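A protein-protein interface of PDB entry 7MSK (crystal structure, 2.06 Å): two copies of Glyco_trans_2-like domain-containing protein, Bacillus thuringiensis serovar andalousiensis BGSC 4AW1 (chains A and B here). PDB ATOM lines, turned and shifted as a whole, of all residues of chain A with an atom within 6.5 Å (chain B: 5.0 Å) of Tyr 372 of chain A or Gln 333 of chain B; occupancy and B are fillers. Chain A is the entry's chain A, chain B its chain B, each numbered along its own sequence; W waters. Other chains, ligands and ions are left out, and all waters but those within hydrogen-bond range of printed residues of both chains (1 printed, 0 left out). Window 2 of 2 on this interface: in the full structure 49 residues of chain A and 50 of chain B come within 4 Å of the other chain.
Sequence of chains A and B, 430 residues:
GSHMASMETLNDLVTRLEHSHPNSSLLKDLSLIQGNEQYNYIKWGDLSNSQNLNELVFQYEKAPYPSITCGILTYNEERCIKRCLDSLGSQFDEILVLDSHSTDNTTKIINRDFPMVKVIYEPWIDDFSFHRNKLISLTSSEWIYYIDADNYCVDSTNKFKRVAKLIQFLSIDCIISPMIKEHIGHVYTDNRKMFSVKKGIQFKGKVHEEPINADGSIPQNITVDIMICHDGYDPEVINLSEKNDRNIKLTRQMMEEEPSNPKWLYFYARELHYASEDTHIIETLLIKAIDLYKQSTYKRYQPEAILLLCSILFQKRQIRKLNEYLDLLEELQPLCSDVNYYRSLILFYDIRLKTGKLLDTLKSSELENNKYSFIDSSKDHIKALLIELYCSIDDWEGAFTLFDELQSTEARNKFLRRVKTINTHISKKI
OD2 of Asp 338 of chain B is in hydrogen-bond range of N of Phe 374 of chain A, 2.8 Å away.
OH of Tyr 372 of chain A is in hydrogen-bond range of OE1 of Gln 333 of chain B.
The backbone carbonyl oxygen of Tyr 372 of chain A is in hydrogen-bond range of the backbone NH of Ser 337 of chain B (2.7 Å).
The side-chain hydroxyl of Ser 373 of chain A is in hydrogen-bond range of the side-chain carboxylate of Asp 338 of chain B, 2.7 Å away.
The backbone NH (N) of Tyr 372 of chain A is in hydrogen-bond range of the backbone carbonyl oxygen (O) of Leu 335 of chain B, 3.1 Å away.
The side-chain hydroxyl (OG) of Ser 337 of chain B lies within hydrogen-bond range of the side-chain carboxylate (OE1) of Glu 366 of chain A (3.4 Å).
The side-chain sulfur (SG) of Cys 336 of chain B lies close to the backbone carbonyl oxygen (O) of Tyr 372 of chain A.
The backbone carbonyl oxygen (O) of Lys 371 of chain A sits at hydrogen-bond distance from the side-chain amino group (NZ) of Lys 379 of chain A, at 2.5 Å.
The side-chain hydroxyl (OG) of Ser 373 of chain A is in hydrogen-bond range of the backbone NH (N) of Asp 376 of chain A (2.9 Å).
NZ of Lys 379 of chain A is in hydrogen-bond range of O of Glu 366 of chain A, 2.8 Å away.
OE1 of Glu 366 of chain A lies within salt-bridge range of NZ of Lys 371 of chain A (3.0 Å).
The side-chain amide oxygen of Asn 369 of chain A sits close to the backbone NH of Lys 371 of chain A (3.5 Å).
The side-chain sulfur (SG) of Cys 336 of chain B sits at hydrogen-bond distance from the side-chain carboxylate (OD2) of Asp 338 of chain B, at 2.8 Å.
Printed residues of chain A that touch a printed residue of chain B: Glu 366, Lys 371, Tyr 372, Ser 373, Phe 374 and Lys 379.
Among the printed residues, no Asp or Glu carboxylate lies within 4 Å of a Lys or Arg side-chain nitrogen of the other chain.
Water W1 lies within hydrogen-bond range of the backbone carbonyl oxygen of Cys 336 of chain B (2.9 Å), the side-chain amino group of Lys 371 of chain A (3.2 Å) and the backbone carbonyl oxygen of Ser 337 of chain B (3.3 Å).
Tyr 372 of chain A touches just these residues of chain B: Gln 333, Leu 335, Cys 336 and Ser 337.
Gln 333 of chain B touches two residues of chain A.
Of the printed residues of chain B, Glu 366 of chain A touches Ser 337.
Of the printed residues of chain A, Leu 335 of chain B touches Lys 371 (3.3 Å) and Tyr 372 (3.1 Å).
The nearest printed residue of chain A that does not touch Gln 333 of chain B is Lys 371 of chain A (6.5 Å).
The nearest printed residue of chain B that does not touch Phe 374 of chain A is Leu 329 of chain B (5.2 Å).
Lys 371 of chain A touches Leu 335 of chain B (CB to O, 3.3 Å).
Ser 337 of chain B touches Lys 371 of chain A.
Pro 303 of chain B touches Phe 374 of chain A.
Phe 374 of chain A touches Gln 333 of chain B.
Phe 374 of chain A touches Cys 336 of chain B.
Ser 337 of chain B touches Lys 379 of chain A.
No position is printed for both chains.
Of the 13 pairs that touch across the chains among the printed residues, none has its exchanged pair printed and touching as well.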
ATOM      1  N   GLU A 366      -8.259  16.285 -22.650  1.00  0.00           N
ATOM      2  CA  GLU A 366      -8.091  15.795 -21.283  1.00  0.00           C
ATOM      3  C   GLU A 366      -8.951  16.512 -20.246  1.00  0.00           C
ATOM      4  O   GLU A 366      -9.096  15.990 -19.142  1.00  0.00           O
ATOM      5  CB  GLU A 366      -6.637  15.905 -20.817  1.00  0.00           C
ATOM      6  CG  GLU A 366      -5.658  15.144 -21.681  1.00  0.00           C
ATOM      7  CD  GLU A 366      -6.102  13.755 -22.103  1.00  0.00           C
ATOM      8  OE1 GLU A 366      -6.893  13.126 -21.374  1.00  0.00           O
ATOM      9  OE2 GLU A 366      -5.645  13.301 -23.161  1.00  0.00           O
ATOM     10  N   ASN A 369     -14.220  15.519 -19.428  1.00  0.00           N
ATOM     11  CA  ASN A 369     -14.638  14.549 -20.432  1.00  0.00           C
ATOM     12  C   ASN A 369     -14.391  13.093 -20.026  1.00  0.00           C
ATOM     13  O   ASN A 369     -14.001  12.286 -20.870  1.00  0.00           O
ATOM     14  CB  ASN A 369     -13.922  14.798 -21.765  1.00  0.00           C
ATOM     15  CG  ASN A 369     -12.418  14.865 -21.616  1.00  0.00           C
ATOM     16  OD1 ASN A 369     -11.830  14.122 -20.831  1.00  0.00           O
ATOM     17  ND2 ASN A 369     -11.788  15.756 -22.363  1.00  0.00           N
ATOM     18  N   ASN A 370     -14.645  12.737 -18.762  1.00  0.00           N
ATOM     19  CA  ASN A 370     -14.698  11.336 -18.359  1.00  0.00           C
ATOM     20  C   ASN A 370     -13.364  10.606 -18.563  1.00  0.00           C
ATOM     21  O   ASN A 370     -13.320   9.378 -18.538  1.00  0.00           O
ATOM     22  CB  ASN A 370     -15.805  10.571 -19.098  1.00  0.00           C
ATOM     23  CG  ASN A 370     -17.206  11.020 -18.734  1.00  0.00           C
ATOM     24  OD1 ASN A 370     -17.409  11.724 -17.745  1.00  0.00           O
ATOM     25  ND2 ASN A 370     -18.186  10.609 -19.526  1.00  0.00           N
ATOM     26  N   LYS A 371     -12.265  11.336 -18.758  1.00  0.00           N
ATOM     27  CA  LYS A 371     -10.951  10.733 -18.605  1.00  0.00           C
ATOM     28  C   LYS A 371     -10.508  11.000 -17.173  1.00  0.00           C
ATOM     29  O   LYS A 371     -10.874  12.025 -16.609  1.00  0.00           O
ATOM     30  CB  LYS A 371      -9.988  11.264 -19.671  1.00  0.00           C
ATOM     31  CG  LYS A 371     -10.359  10.860 -21.092  1.00  0.00           C
ATOM     32  CD  LYS A 371      -9.279  11.117 -22.110  1.00  0.00           C
ATOM     33  CE  LYS A 371      -8.165  10.093 -22.069  1.00  0.00           C
ATOM     34  NZ  LYS A 371      -6.973  10.550 -22.827  1.00  0.00           N
ATOM     35  N   TYR A 372      -9.776  10.055 -16.573  1.00  0.00           N
ATOM     36  CA  TYR A 372      -9.448  10.138 -15.157  1.00  0.00           C
ATOM     37  C   TYR A 372      -7.934  10.147 -14.962  1.00  0.00           C
ATOM     38  O   TYR A 372      -7.170   9.691 -15.817  1.00  0.00           O
ATOM     39  CB  TYR A 372     -10.082   8.992 -14.364  1.00  0.00           C
ATOM     40  CG  TYR A 372      -9.874   7.632 -14.978  1.00  0.00           C
ATOM     41  CD1 TYR A 372      -8.753   6.880 -14.680  1.00  0.00           C
ATOM     42  CD2 TYR A 372     -10.782   7.107 -15.880  1.00  0.00           C
ATOM     43  CE1 TYR A 372      -8.540   5.642 -15.259  1.00  0.00           C
ATOM     44  CE2 TYR A 372     -10.591   5.867 -16.465  1.00  0.00           C
ATOM     45  CZ  TYR A 372      -9.461   5.132 -16.154  1.00  0.00           C
ATOM     46  OH  TYR A 372      -9.241   3.910 -16.728  1.00  0.00           O
ATOM     47  N   SER A 373      -7.530  10.662 -13.797  1.00  0.00           N
ATOM     48  CA  SER A 373      -6.138  10.737 -13.405  1.00  0.00           C
ATOM     49  C   SER A 373      -5.906   9.981 -12.098  1.00  0.00           C
ATOM     50  O   SER A 373      -6.757   9.996 -11.210  1.00  0.00           O
ATOM     51  CB  SER A 373      -5.729  12.160 -13.261  1.00  0.00           C
ATOM     52  OG  SER A 373      -4.495  12.238 -12.568  1.00  0.00           O
ATOM     53  N   PHE A 374      -4.737   9.335 -12.001  1.00  0.00           N
ATOM     54  CA  PHE A 374      -4.238   8.778 -10.759  1.00  0.00           C
ATOM     55  C   PHE A 374      -3.239   9.720 -10.097  1.00  0.00           C
ATOM     56  O   PHE A 374      -2.687   9.372  -9.056  1.00  0.00           O
ATOM     57  CB  PHE A 374      -3.538   7.443 -11.016  1.00  0.00           C
ATOM     58  CG  PHE A 374      -4.421   6.417 -11.671  1.00  0.00           C
ATOM     59  CD1 PHE A 374      -5.218   5.577 -10.908  1.00  0.00           C
ATOM     60  CD2 PHE A 374      -4.469   6.308 -13.051  1.00  0.00           C
ATOM     61  CE1 PHE A 374      -6.032   4.631 -11.519  1.00  0.00           C
ATOM     62  CE2 PHE A 374      -5.284   5.370 -13.662  1.00  0.00           C
ATOM     63  CZ  PHE A 374      -6.068   4.533 -12.896  1.00  0.00           C
ATOM     64  N   ASP A 376      -3.873  13.437  -9.970  1.00  0.00           N
ATOM     65  CA  ASP A 376      -4.737  14.412  -9.331  1.00  0.00           C
ATOM     66  C   ASP A 376      -6.096  14.384 -10.021  1.00  0.00           C
ATOM     67  O   ASP A 376      -6.198  14.737 -11.192  1.00  0.00           O
ATOM     68  CB  ASP A 376      -4.106  15.804  -9.389  1.00  0.00           C
ATOM     69  CG  ASP A 376      -4.931  16.859  -8.681  1.00  0.00           C
ATOM     70  OD1 ASP A 376      -6.128  16.591  -8.426  1.00  0.00           O
ATOM     71  OD2 ASP A 376      -4.371  17.932  -8.392  1.00  0.00           O
ATOM     72  N   SER A 377      -7.134  13.985  -9.274  1.00  0.00           N
ATOM     73  CA  SER A 377      -8.464  13.767  -9.826  1.00  0.00           C
ATOM     74  C   SER A 377      -9.070  15.051 -10.383  1.00  0.00           C
ATOM     75  O   SER A 377      -9.814  14.976 -11.347  1.00  0.00           O
ATOM     76  CB  SER A 377      -9.390  13.142  -8.812  1.00  0.00           C
ATOM     77  OG  SER A 377      -9.338  11.729  -8.903  1.00  0.00           O
ATOM     78  N   LYS A 379      -7.406  17.267 -11.934  1.00  0.00           N
ATOM     79  CA  LYS A 379      -6.647  17.564 -13.144  1.00  0.00           C
ATOM     80  C   LYS A 379      -5.878  18.889 -13.032  1.00  0.00           C
ATOM     81  O   LYS A 379      -5.555  19.501 -14.049  1.00  0.00           O
ATOM     82  CB  LYS A 379      -7.572  17.486 -14.367  1.00  0.00           C
ATOM     83  CG  LYS A 379      -8.146  16.095 -14.621  1.00  0.00           C
ATOM     84  CD  LYS A 379      -8.973  15.976 -15.884  1.00  0.00           C
ATOM     85  CE  LYS A 379      -9.693  14.644 -15.962  1.00  0.00           C
ATOM     86  NZ  LYS A 379     -10.396  14.444 -17.252  1.00  0.00           N
ATOM     87  N   PRO B 303      -1.097   1.593 -11.658  1.00  0.00           N
ATOM     88  CA  PRO B 303      -1.001   2.884 -12.330  1.00  0.00           C
ATOM     89  C   PRO B 303      -0.093   3.849 -11.571  1.00  0.00           C
ATOM     90  O   PRO B 303       0.744   4.515 -12.180  1.00  0.00           O
ATOM     91  CB  PRO B 303      -2.459   3.384 -12.370  1.00  0.00           C
ATOM     92  CG  PRO B 303      -3.303   2.123 -12.240  1.00  0.00           C
ATOM     93  CD  PRO B 303      -2.489   1.219 -11.343  1.00  0.00           C
ATOM     94  N   LEU B 329       1.052   2.000 -19.792  1.00  0.00           N
ATOM     95  CA  LEU B 329      -0.038   2.564 -19.002  1.00  0.00           C
ATOM     96  C   LEU B 329      -1.259   2.808 -19.887  1.00  0.00           C
ATOM     97  O   LEU B 329      -2.390   2.586 -19.460  1.00  0.00           O
ATOM     98  CB  LEU B 329       0.421   3.862 -18.317  1.00  0.00           C
ATOM     99  CG  LEU B 329      -0.654   4.618 -17.532  1.00  0.00           C
ATOM    100  CD1 LEU B 329      -1.181   3.766 -16.380  1.00  0.00           C
ATOM    101  CD2 LEU B 329      -0.133   5.951 -17.009  1.00  0.00           C
ATOM    102  N   GLU B 330      -1.027   3.303 -21.106  1.00  0.00           N
ATOM    103  CA  GLU B 330      -2.096   3.534 -22.069  1.00  0.00           C
ATOM    104  C   GLU B 330      -2.863   2.235 -22.320  1.00  0.00           C
ATOM    105  O   GLU B 330      -4.078   2.244 -22.431  1.00  0.00           O
ATOM    106  CB  GLU B 330      -1.515   4.079 -23.376  1.00  0.00           C
ATOM    107  CG  GLU B 330      -2.571   4.513 -24.382  1.00  0.00           C
ATOM    108  CD  GLU B 330      -2.039   5.470 -25.437  1.00  0.00           C
ATOM    109  OE1 GLU B 330      -0.875   5.322 -25.815  1.00  0.00           O
ATOM    110  OE2 GLU B 330      -2.774   6.383 -25.849  1.00  0.00           O
ATOM    111  N   GLU B 331      -2.137   1.120 -22.414  1.00  0.00           N
ATOM    112  CA  GLU B 331      -2.730  -0.188 -22.659  1.00  0.00           C
ATOM    113  C   GLU B 331      -3.581  -0.603 -21.455  1.00  0.00           C
ATOM    114  O   GLU B 331      -4.726  -1.004 -21.633  1.00  0.00           O
ATOM    115  CB  GLU B 331      -1.610  -1.186 -22.977  1.00  0.00           C
ATOM    116  CG  GLU B 331      -2.071  -2.603 -23.228  1.00  0.00           C
ATOM    117  CD  GLU B 331      -1.018  -3.457 -23.911  1.00  0.00           C
ATOM    118  OE1 GLU B 331       0.197  -3.243 -23.645  1.00  0.00           O
ATOM    119  OE2 GLU B 331      -1.410  -4.313 -24.726  1.00  0.00           O
ATOM    120  N   LEU B 332      -3.030  -0.471 -20.236  1.00  0.00           N
ATOM    121  CA  LEU B 332      -3.724  -0.880 -19.019  1.00  0.00           C
ATOM    122  C   LEU B 332      -4.913   0.037 -18.726  1.00  0.00           C
ATOM    123  O   LEU B 332      -5.900  -0.435 -18.171  1.00  0.00           O
ATOM    124  CB  LEU B 332      -2.762  -0.884 -17.821  1.00  0.00           C
ATOM    125  CG  LEU B 332      -1.542  -1.804 -17.921  1.00  0.00           C
ATOM    126  CD1 LEU B 332      -0.590  -1.548 -16.760  1.00  0.00           C
ATOM    127  CD2 LEU B 332      -1.935  -3.273 -17.982  1.00  0.00           C
ATOM    128  N   GLN B 333      -4.818   1.336 -19.063  1.00  0.00           N
ATOM    129  CA  GLN B 333      -5.804   2.314 -18.618  1.00  0.00           C
ATOM    130  C   GLN B 333      -6.154   3.272 -19.753  1.00  0.00           C
ATOM    131  O   GLN B 333      -5.883   4.472 -19.679  1.00  0.00           O
ATOM    132  CB  GLN B 333      -5.287   3.087 -17.405  1.00  0.00           C
ATOM    133  CG  GLN B 333      -5.000   2.204 -16.199  1.00  0.00           C
ATOM    134  CD  GLN B 333      -6.231   1.864 -15.402  1.00  0.00           C
ATOM    135  OE1 GLN B 333      -7.295   2.448 -15.578  1.00  0.00           O
ATOM    136  NE2 GLN B 333      -6.087   0.921 -14.489  1.00  0.00           N
ATOM    137  N   PRO B 334      -6.852   2.783 -20.803  1.00  0.00           N
ATOM    138  CA  PRO B 334      -7.073   3.563 -22.023  1.00  0.00           C
ATOM    139  C   PRO B 334      -7.512   5.006 -21.810  1.00  0.00           C
ATOM    140  O   PRO B 334      -7.167   5.878 -22.602  1.00  0.00           O
ATOM    141  CB  PRO B 334      -8.203   2.787 -22.717  1.00  0.00           C
ATOM    142  CG  PRO B 334      -7.960   1.362 -22.304  1.00  0.00           C
ATOM    143  CD  PRO B 334      -7.489   1.459 -20.867  1.00  0.00           C
ATOM    144  N   LEU B 335      -8.283   5.247 -20.749  1.00  0.00           N
ATOM    145  CA  LEU B 335      -8.908   6.544 -20.556  1.00  0.00           C
ATOM    146  C   LEU B 335      -8.199   7.345 -19.464  1.00  0.00           C
ATOM    147  O   LEU B 335      -8.751   8.336 -18.989  1.00  0.00           O
ATOM    148  CB  LEU B 335     -10.384   6.316 -20.217  1.00  0.00           C
ATOM    149  CG  LEU B 335     -11.195   5.571 -21.280  1.00  0.00           C
ATOM    150  CD1 LEU B 335     -12.404   4.885 -20.660  1.00  0.00           C
ATOM    151  CD2 LEU B 335     -11.625   6.510 -22.399  1.00  0.00           C
ATOM    152  N   CYS B 336      -6.976   6.938 -19.088  1.00  0.00           N
ATOM    153  CA  CYS B 336      -6.205   7.675 -18.100  1.00  0.00           C
ATOM    154  C   CYS B 336      -5.569   8.927 -18.706  1.00  0.00           C
ATOM    155  O   CYS B 336      -4.801   8.820 -19.664  1.00  0.00           O
ATOM    156  CB  CYS B 336      -5.085   6.817 -17.531  1.00  0.00           C
ATOM    157  SG  CYS B 336      -4.107   7.699 -16.285  1.00  0.00           S
ATOM    158  N   SER B 337      -5.830  10.098 -18.103  1.00  0.00           N
ATOM    159  CA  SER B 337      -5.379  11.381 -18.636  1.00  0.00           C
ATOM    160  C   SER B 337      -3.868  11.562 -18.504  1.00  0.00           C
ATOM    161  O   SER B 337      -3.299  12.431 -19.148  1.00  0.00           O
ATOM    162  CB  SER B 337      -6.065  12.539 -17.954  1.00  0.00           C
ATOM    163  OG  SER B 337      -7.477  12.494 -18.123  1.00  0.00           O
ATOM    164  N   ASP B 338      -3.233  10.788 -17.623  1.00  0.00           N
ATOM    165  CA  ASP B 338      -1.855  11.038 -17.234  1.00  0.00           C
ATOM    166  C   ASP B 338      -0.890  10.702 -18.368  1.00  0.00           C
ATOM    167  O   ASP B 338       0.238  11.186 -18.381  1.00  0.00           O
ATOM    168  CB  ASP B 338      -1.547  10.270 -15.948  1.00  0.00           C
ATOM    169  CG  ASP B 338      -2.590  10.549 -14.880  1.00  0.00           C
ATOM    170  OD1 ASP B 338      -2.822  11.733 -14.604  1.00  0.00           O
ATOM    171  OD2 ASP B 338      -3.213   9.577 -14.391  1.00  0.00           O
HETATM  172  O   HOH W   1      -3.892  10.530 -21.805  1.00  0.00           O
